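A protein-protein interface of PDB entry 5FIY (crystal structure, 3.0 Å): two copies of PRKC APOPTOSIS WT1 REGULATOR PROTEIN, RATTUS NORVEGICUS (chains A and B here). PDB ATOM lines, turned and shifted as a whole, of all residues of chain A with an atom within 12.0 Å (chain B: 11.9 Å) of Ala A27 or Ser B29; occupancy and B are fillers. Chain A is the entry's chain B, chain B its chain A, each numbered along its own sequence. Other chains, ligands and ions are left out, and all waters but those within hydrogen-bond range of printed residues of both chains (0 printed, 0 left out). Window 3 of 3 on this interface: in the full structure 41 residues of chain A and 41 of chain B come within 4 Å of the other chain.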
ATOM      1  N   ALA A  27      15.906   0.122 -16.364  1.00  0.00           N
ATOM      2  CA  ALA A  27      16.921  -0.926 -16.347  1.00  0.00           C
ATOM      3  C   ALA A  27      16.323  -2.287 -16.675  1.00  0.00           C
ATOM      4  O   ALA A  27      15.555  -2.843 -15.885  1.00  0.00           O
ATOM      5  CB  ALA A  27      17.615  -0.969 -14.995  1.00  0.00           C
ATOM      6  N   SER A  28      16.680  -2.828 -17.836  1.00  0.00           N
ATOM      7  CA  SER A  28      16.108  -4.092 -18.272  1.00  0.00           C
ATOM      8  C   SER A  28      16.879  -5.231 -17.619  1.00  0.00           C
ATOM      9  O   SER A  28      18.089  -5.128 -17.394  1.00  0.00           O
ATOM     10  CB  SER A  28      16.136  -4.214 -19.799  1.00  0.00           C
ATOM     11  OG  SER A  28      17.462  -4.174 -20.302  1.00  0.00           O
ATOM     12  N   SER A  29      16.172  -6.318 -17.329  1.00  0.00           N
ATOM     13  CA  SER A  29      16.753  -7.471 -16.648  1.00  0.00           C
ATOM     14  C   SER A  29      17.882  -8.124 -17.439  1.00  0.00           C
ATOM     15  O   SER A  29      18.807  -8.675 -16.855  1.00  0.00           O
ATOM     16  CB  SER A  29      15.668  -8.502 -16.332  1.00  0.00           C
ATOM     17  OG  SER A  29      15.100  -8.256 -15.053  1.00  0.00           O
ATOM     18  N   SER A  30      17.806  -8.076 -18.763  1.00  0.00           N
ATOM     19  CA  SER A  30      18.858  -8.660 -19.588  1.00  0.00           C
ATOM     20  C   SER A  30      20.161  -7.878 -19.432  1.00  0.00           C
ATOM     21  O   SER A  30      21.235  -8.460 -19.239  1.00  0.00           O
ATOM     22  CB  SER A  30      18.429  -8.695 -21.056  1.00  0.00           C
ATOM     23  OG  SER A  30      18.219  -7.387 -21.558  1.00  0.00           O
ATOM     24  N   THR A  31      20.055  -6.554 -19.500  1.00  0.00           N
ATOM     25  CA  THR A  31      21.203  -5.676 -19.312  1.00  0.00           C
ATOM     26  C   THR A  31      21.814  -5.864 -17.923  1.00  0.00           C
ATOM     27  O   THR A  31      23.032  -5.950 -17.786  1.00  0.00           O
ATOM     28  CB  THR A  31      20.826  -4.193 -19.525  1.00  0.00           C
ATOM     29  OG1 THR A  31      20.789  -3.907 -20.930  1.00  0.00           O
ATOM     30  CG2 THR A  31      21.840  -3.272 -18.858  1.00  0.00           C
ATOM     31  N   LEU A  32      20.967  -5.922 -16.898  1.00  0.00           N
ATOM     32  CA  LEU A  32      21.439  -6.160 -15.535  1.00  0.00           C
ATOM     33  C   LEU A  32      22.150  -7.508 -15.386  1.00  0.00           C
ATOM     34  O   LEU A  32      23.222  -7.596 -14.781  1.00  0.00           O
ATOM     35  CB  LEU A  32      20.272  -6.082 -14.549  1.00  0.00           C
ATOM     36  CG  LEU A  32      19.601  -4.720 -14.345  1.00  0.00           C
ATOM     37  CD1 LEU A  32      18.741  -4.727 -13.089  1.00  0.00           C
ATOM     38  CD2 LEU A  32      20.636  -3.607 -14.271  1.00  0.00           C
ATOM     39  N   GLU A  33      21.554  -8.551 -15.954  1.00  0.00           N
ATOM     40  CA  GLU A  33      22.123  -9.891 -15.882  1.00  0.00           C
ATOM     41  C   GLU A  33      23.472  -9.938 -16.584  1.00  0.00           C
ATOM     42  O   GLU A  33      24.409 -10.608 -16.123  1.00  0.00           O
ATOM     43  CB  GLU A  33      21.161 -10.920 -16.491  1.00  0.00           C
ATOM     44  CG  GLU A  33      19.998 -11.310 -15.579  1.00  0.00           C
ATOM     45  CD  GLU A  33      19.169 -12.459 -16.133  1.00  0.00           C
ATOM     46  OE1 GLU A  33      19.639 -13.136 -17.074  1.00  0.00           O
ATOM     47  OE2 GLU A  33      18.045 -12.679 -15.631  1.00  0.00           O
ATOM     48  N   LYS A  34      23.591  -9.189 -17.676  1.00  0.00           N
ATOM     49  CA  LYS A  34      24.862  -9.156 -18.381  1.00  0.00           C
ATOM     50  C   LYS A  34      25.892  -8.361 -17.586  1.00  0.00           C
ATOM     51  O   LYS A  34      27.065  -8.729 -17.555  1.00  0.00           O
ATOM     52  CB  LYS A  34      24.726  -8.565 -19.786  1.00  0.00           C
ATOM     53  CG  LYS A  34      26.066  -8.568 -20.511  1.00  0.00           C
ATOM     54  CD  LYS A  34      25.982  -8.222 -21.971  1.00  0.00           C
ATOM     55  CE  LYS A  34      27.340  -8.453 -22.604  1.00  0.00           C
ATOM     56  NZ  LYS A  34      27.997  -9.664 -22.024  1.00  0.00           N
ATOM     57  N   ARG A  35      25.460  -7.272 -16.957  1.00  0.00           N
ATOM     58  CA  ARG A  35      26.338  -6.504 -16.084  1.00  0.00           C
ATOM     59  C   ARG A  35      26.912  -7.393 -14.996  1.00  0.00           C
ATOM     60  O   ARG A  35      28.112  -7.341 -14.702  1.00  0.00           O
ATOM     61  CB  ARG A  35      25.588  -5.331 -15.460  1.00  0.00           C
ATOM     62  CG  ARG A  35      26.437  -4.513 -14.516  1.00  0.00           C
ATOM     63  CD  ARG A  35      27.519  -3.793 -15.284  1.00  0.00           C
ATOM     64  NE  ARG A  35      28.273  -2.879 -14.435  1.00  0.00           N
ATOM     65  CZ  ARG A  35      29.277  -2.124 -14.865  1.00  0.00           C
ATOM     66  NH1 ARG A  35      29.652  -2.171 -16.141  1.00  0.00           N
ATOM     67  NH2 ARG A  35      29.907  -1.325 -14.016  1.00  0.00           N
ATOM     68  N   ILE A  36      26.050  -8.224 -14.417  1.00  0.00           N
ATOM     69  CA  ILE A  36      26.484  -9.176 -13.404  1.00  0.00           C
ATOM     70  C   ILE A  36      27.479 -10.188 -13.970  1.00  0.00           C
ATOM     71  O   ILE A  36      28.511 -10.467 -13.354  1.00  0.00           O
ATOM     72  CB  ILE A  36      25.286  -9.913 -12.784  1.00  0.00           C
ATOM     73  CG1 ILE A  36      24.489  -8.950 -11.900  1.00  0.00           C
ATOM     74  CG2 ILE A  36      25.749 -11.104 -11.952  1.00  0.00           C
ATOM     75  CD1 ILE A  36      23.204  -9.524 -11.343  1.00  0.00           C
ATOM     76  N   LEU A  39      30.864  -8.310 -14.557  1.00  0.00           N
ATOM     77  CA  LEU A  39      31.515  -8.003 -13.288  1.00  0.00           C
ATOM     78  C   LEU A  39      32.074  -9.244 -12.613  1.00  0.00           C
ATOM     79  O   LEU A  39      33.136  -9.185 -12.001  1.00  0.00           O
ATOM     80  CB  LEU A  39      30.546  -7.292 -12.347  1.00  0.00           C
ATOM     81  CG  LEU A  39      30.275  -5.842 -12.744  1.00  0.00           C
ATOM     82  CD1 LEU A  39      29.202  -5.231 -11.858  1.00  0.00           C
ATOM     83  CD2 LEU A  39      31.562  -5.031 -12.695  1.00  0.00           C
ATOM     84  N   PHE B  26      14.253 -16.458 -11.492  1.00  0.00           N
ATOM     85  CA  PHE B  26      13.989 -15.037 -11.700  1.00  0.00           C
ATOM     86  C   PHE B  26      14.475 -14.185 -10.533  1.00  0.00           C
ATOM     87  O   PHE B  26      14.387 -14.592  -9.372  1.00  0.00           O
ATOM     88  CB  PHE B  26      12.492 -14.788 -11.922  1.00  0.00           C
ATOM     89  CG  PHE B  26      12.088 -13.345 -11.775  1.00  0.00           C
ATOM     90  CD1 PHE B  26      12.184 -12.468 -12.846  1.00  0.00           C
ATOM     91  CD2 PHE B  26      11.614 -12.864 -10.560  1.00  0.00           C
ATOM     92  CE1 PHE B  26      11.818 -11.140 -12.703  1.00  0.00           C
ATOM     93  CE2 PHE B  26      11.253 -11.542 -10.413  1.00  0.00           C
ATOM     94  CZ  PHE B  26      11.353 -10.679 -11.483  1.00  0.00           C
ATOM     95  N   ALA B  27      14.979 -12.996 -10.846  1.00  0.00           N
ATOM     96  CA  ALA B  27      15.461 -12.091  -9.815  1.00  0.00           C
ATOM     97  C   ALA B  27      14.956 -10.669 -10.028  1.00  0.00           C
ATOM     98  O   ALA B  27      14.889 -10.182 -11.161  1.00  0.00           O
ATOM     99  CB  ALA B  27      16.975 -12.112  -9.765  1.00  0.00           C
ATOM    100  N   SER B  28      14.626 -10.010  -8.920  1.00  0.00           N
ATOM    101  CA  SER B  28      14.062  -8.665  -8.929  1.00  0.00           C
ATOM    102  C   SER B  28      15.029  -7.690  -9.576  1.00  0.00           C
ATOM    103  O   SER B  28      16.240  -7.916  -9.560  1.00  0.00           O
ATOM    104  CB  SER B  28      13.748  -8.196  -7.504  1.00  0.00           C
ATOM    105  OG  SER B  28      13.155  -9.225  -6.731  1.00  0.00           O
ATOM    106  N   SER B  29      14.505  -6.628 -10.181  1.00  0.00           N
ATOM    107  CA  SER B  29      15.381  -5.637 -10.779  1.00  0.00           C
ATOM    108  C   SER B  29      16.236  -5.070  -9.657  1.00  0.00           C
ATOM    109  O   SER B  29      17.420  -4.821  -9.839  1.00  0.00           O
ATOM    110  CB  SER B  29      14.594  -4.528 -11.485  1.00  0.00           C
ATOM    111  OG  SER B  29      14.370  -4.849 -12.848  1.00  0.00           O
ATOM    112  N   SER B  30      15.641  -4.944  -8.475  1.00  0.00           N
ATOM    113  CA  SER B  30      16.346  -4.454  -7.295  1.00  0.00           C
ATOM    114  C   SER B  30      17.409  -5.447  -6.830  1.00  0.00           C
ATOM    115  O   SER B  30      18.517  -5.056  -6.464  1.00  0.00           O
ATOM    116  CB  SER B  30      15.360  -4.167  -6.159  1.00  0.00           C
ATOM    117  OG  SER B  30      14.688  -5.347  -5.749  1.00  0.00           O
ATOM    118  N   THR B  31      17.053  -6.727  -6.819  1.00  0.00           N
ATOM    119  CA  THR B  31      17.977  -7.783  -6.426  1.00  0.00           C
ATOM    120  C   THR B  31      19.218  -7.791  -7.315  1.00  0.00           C
ATOM    121  O   THR B  31      20.361  -7.836  -6.829  1.00  0.00           O
ATOM    122  CB  THR B  31      17.283  -9.158  -6.493  1.00  0.00           C
ATOM    123  OG1 THR B  31      16.480  -9.343  -5.322  1.00  0.00           O
ATOM    124  CG2 THR B  31      18.296 -10.285  -6.591  1.00  0.00           C
ATOM    125  N   LEU B  32      18.980  -7.719  -8.618  1.00  0.00           N
ATOM    126  CA  LEU B  32      20.049  -7.629  -9.598  1.00  0.00           C
ATOM    127  C   LEU B  32      20.869  -6.367  -9.359  1.00  0.00           C
ATOM    128  O   LEU B  32      22.101  -6.398  -9.425  1.00  0.00           O
ATOM    129  CB  LEU B  32      19.474  -7.649 -11.017  1.00  0.00           C
ATOM    130  CG  LEU B  32      18.823  -8.975 -11.413  1.00  0.00           C
ATOM    131  CD1 LEU B  32      18.627  -9.061 -12.914  1.00  0.00           C
ATOM    132  CD2 LEU B  32      19.671 -10.132 -10.922  1.00  0.00           C
ATOM    133  N   GLU B  33      20.181  -5.265  -9.054  1.00  0.00           N
ATOM    134  CA  GLU B  33      20.846  -3.989  -8.819  1.00  0.00           C
ATOM    135  C   GLU B  33      21.805  -4.107  -7.640  1.00  0.00           C
ATOM    136  O   GLU B  33      22.906  -3.546  -7.664  1.00  0.00           O
ATOM    137  CB  GLU B  33      19.826  -2.875  -8.520  1.00  0.00           C
ATOM    138  CG  GLU B  33      19.016  -2.321  -9.705  1.00  0.00           C
ATOM    139  CD  GLU B  33      19.837  -1.686 -10.814  1.00  0.00           C
ATOM    140  OE1 GLU B  33      21.060  -1.504 -10.642  1.00  0.00           O
ATOM    141  OE2 GLU B  33      19.243  -1.361 -11.867  1.00  0.00           O
ATOM    142  N   LYS B  34      21.402  -4.863  -6.619  1.00  0.00           N
ATOM    143  CA  LYS B  34      22.264  -5.036  -5.459  1.00  0.00           C
ATOM    144  C   LYS B  34      23.416  -5.995  -5.739  1.00  0.00           C
ATOM    145  O   LYS B  34      24.518  -5.770  -5.259  1.00  0.00           O
ATOM    146  CB  LYS B  34      21.496  -5.520  -4.232  1.00  0.00           C
ATOM    147  CG  LYS B  34      22.414  -5.594  -3.021  1.00  0.00           C
ATOM    148  CD  LYS B  34      21.712  -5.842  -1.713  1.00  0.00           C
ATOM    149  CE  LYS B  34      22.708  -5.661  -0.572  1.00  0.00           C
ATOM    150  NZ  LYS B  34      23.888  -6.573  -0.684  1.00  0.00           N
ATOM    151  N   ARG B  35      23.172  -7.074  -6.482  1.00  0.00           N
ATOM    152  CA  ARG B  35      24.279  -7.951  -6.869  1.00  0.00           C
ATOM    153  C   ARG B  35      25.335  -7.133  -7.609  1.00  0.00           C
ATOM    154  O   ARG B  35      26.541  -7.297  -7.391  1.00  0.00           O
ATOM    155  CB  ARG B  35      23.797  -9.120  -7.730  1.00  0.00           C
ATOM    156  CG  ARG B  35      24.915 -10.055  -8.188  1.00  0.00           C
ATOM    157  CD  ARG B  35      25.527 -10.842  -7.022  1.00  0.00           C
ATOM    158  NE  ARG B  35      26.476 -11.853  -7.490  1.00  0.00           N
ATOM    159  CZ  ARG B  35      27.157 -12.678  -6.695  1.00  0.00           C
ATOM    160  NH1 ARG B  35      27.003 -12.625  -5.378  1.00  0.00           N
ATOM    161  NH2 ARG B  35      27.996 -13.561  -7.219  1.00  0.00           N
ATOM    162  N   ILE B  36      24.866  -6.244  -8.481  1.00  0.00           N
ATOM    163  CA  ILE B  36      25.752  -5.349  -9.219  1.00  0.00           C
ATOM    164  C   ILE B  36      26.514  -4.407  -8.274  1.00  0.00           C
ATOM    165  O   ILE B  36      27.732  -4.219  -8.410  1.00  0.00           O
ATOM    166  CB  ILE B  36      24.962  -4.535 -10.259  1.00  0.00           C
ATOM    167  CG1 ILE B  36      24.467  -5.464 -11.371  1.00  0.00           C
ATOM    168  CG2 ILE B  36      25.820  -3.431 -10.837  1.00  0.00           C
ATOM    169  CD1 ILE B  36      23.555  -4.817 -12.382  1.00  0.00           C
ATOM    170  N   GLU B  37      25.790  -3.840  -7.309  1.00  0.00           N
ATOM    171  CA  GLU B  37      26.367  -2.953  -6.294  1.00  0.00           C
ATOM    172  C   GLU B  37      27.529  -3.628  -5.559  1.00  0.00           C
ATOM    173  O   GLU B  37      28.655  -3.099  -5.457  1.00  0.00           O
ATOM    174  CB  GLU B  37      25.273  -2.574  -5.285  1.00  0.00           C
ATOM    175  CG  GLU B  37      25.115  -1.103  -4.955  1.00  0.00           C
ATOM    176  CD  GLU B  37      23.888  -0.853  -4.088  1.00  0.00           C
ATOM    177  OE1 GLU B  37      22.760  -0.924  -4.624  1.00  0.00           O
ATOM    178  OE2 GLU B  37      24.048  -0.605  -2.872  1.00  0.00           O
ATOM    179  N   ASP B  38      27.232  -4.836  -5.088  1.00  0.00           N
ATOM    180  CA  ASP B  38      28.143  -5.657  -4.312  1.00  0.00           C
ATOM    181  C   ASP B  38      29.373  -6.027  -5.119  1.00  0.00           C
ATOM    182  O   ASP B  38      30.500  -5.888  -4.640  1.00  0.00           O
ATOM    183  CB  ASP B  38      27.426  -6.918  -3.827  1.00  0.00           C
ATOM    184  CG  ASP B  38      26.435  -6.633  -2.712  1.00  0.00           C
ATOM    185  OD1 ASP B  38      26.475  -5.521  -2.139  1.00  0.00           O
ATOM    186  OD2 ASP B  38      25.612  -7.520  -2.406  1.00  0.00           O
ATOM    187  N   GLU B  40      30.554  -4.496  -7.693  1.00  0.00           N
ATOM    188  CA  GLU B  40      31.351  -3.311  -7.988  1.00  0.00           C
ATOM    189  C   GLU B  40      32.215  -2.935  -6.781  1.00  0.00           C
ATOM    190  O   GLU B  40      33.420  -2.635  -6.931  1.00  0.00           O
ATOM    191  CB  GLU B  40      30.448  -2.158  -8.422  1.00  0.00           C
ATOM    192  CG  GLU B  40      29.981  -2.324  -9.865  1.00  0.00           C
ATOM    193  CD  GLU B  40      29.159  -1.167 -10.387  1.00  0.00           C
ATOM    194  OE1 GLU B  40      29.262  -0.058  -9.822  1.00  0.00           O
ATOM    195  OE2 GLU B  40      28.416  -1.372 -11.371  1.00  0.00           O
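Of the 11 printed residues of chain A, 7 touch a printed residue of chain B.
Hydrophobic or aromatic side chains of chain A within 4 Å of the printed part of chain B: Ala A27, Leu A32, Ile A36 and Leu A39.
Among the printed residues, Asp or Glu carboxylates within 4 Å of a Lys or Arg side-chain nitrogen of the other chain: Arg A35 with Glu B40 (3.0 Å).
Of the printed residues of chain B, Ala A27 touches Ser B29 (3.8 Å) and Glu B33 (3.5 Å).
Ser A28 touches none of the printed residues of chain B.
Ser A29 touches one residue of chain B.
Ser A30 touches none of the printed residues of chain B.
No residue of chain B comes within 4 Å of Thr A31.
Of the printed residues of chain B, Leu A32 touches Ser B29, Leu B32, Glu B33 and Ile B36.
Of the printed residues of chain B, Arg A35 touches Ile B36 (3.6 Å) and Glu B40 (3.0 Å).
Printed residues of chain B within 4 Å of Leu A39: Ile B36 (3.9 Å) and Glu B40 (3.6 Å).
No residue of chain A comes within 4 Å of Ala B27.
No residue of chain A comes within 4 Å of Ser B28.
Ser B29 touches two residues of chain A.
No residue of chain A comes within 4 Å of Ser B30.
Of chain A, only Ser A29, Leu A32, Glu A33 and Ile A36 come within 4 Å of Leu B32.
Of the printed residues of chain A, Arg B35 touches Ile A36 (3.6 Å).
Asp B38 touches none of the printed residues of chain A.
The nearest printed residue of chain B that does not touch Ala A27 is Ile B36 (7.5 Å).
The nearest residue of chain A that does not touch Ser B29 is Ser A29 (4.1 Å).
OE2 of Glu B40 is in salt-bridge range of NH2 of Arg A35 (3.0 Å).
Among the printed residues, pairs that only touch across the chains: Ala A27 with Ser B29 (3.8 Å), Ala A27 with Glu B33 (3.5 Å), Ser A29 with Leu B32 (3.96 Å), Leu A32 with Ser B29 (3.5 Å), Leu A32 with Leu B32 (3.7 Å), Leu A32 with Glu B33 (3.6 Å), Leu A32 with Ile B36 (3.7 Å), Glu A33 with Leu B32 (3.7 Å), Arg A35 with Ile B36 (3.6 Å), Ile A36 with Leu B32 (3.6 Å), Ile A36 with Arg B35 (3.6 Å), Ile A36 with Ile B36 (3.5 Å), Leu A39 with Ile B36 (3.9 Å) and Leu A39 with Glu B40 (3.6 Å).
Ala A27 touches Glu B33, but with the chains exchanged Glu A33 does not touch Ala B27 (5.7 Å).
Ser A29 touches Leu B32, and with the chains exchanged Leu A32 touches Ser B29.
Leu A32 touches Ile B36, and with the chains exchanged Ile A36 touches Leu B32.
Arg A35 touches Ile B36, and with the chains exchanged Ile A36 touches Arg B35.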
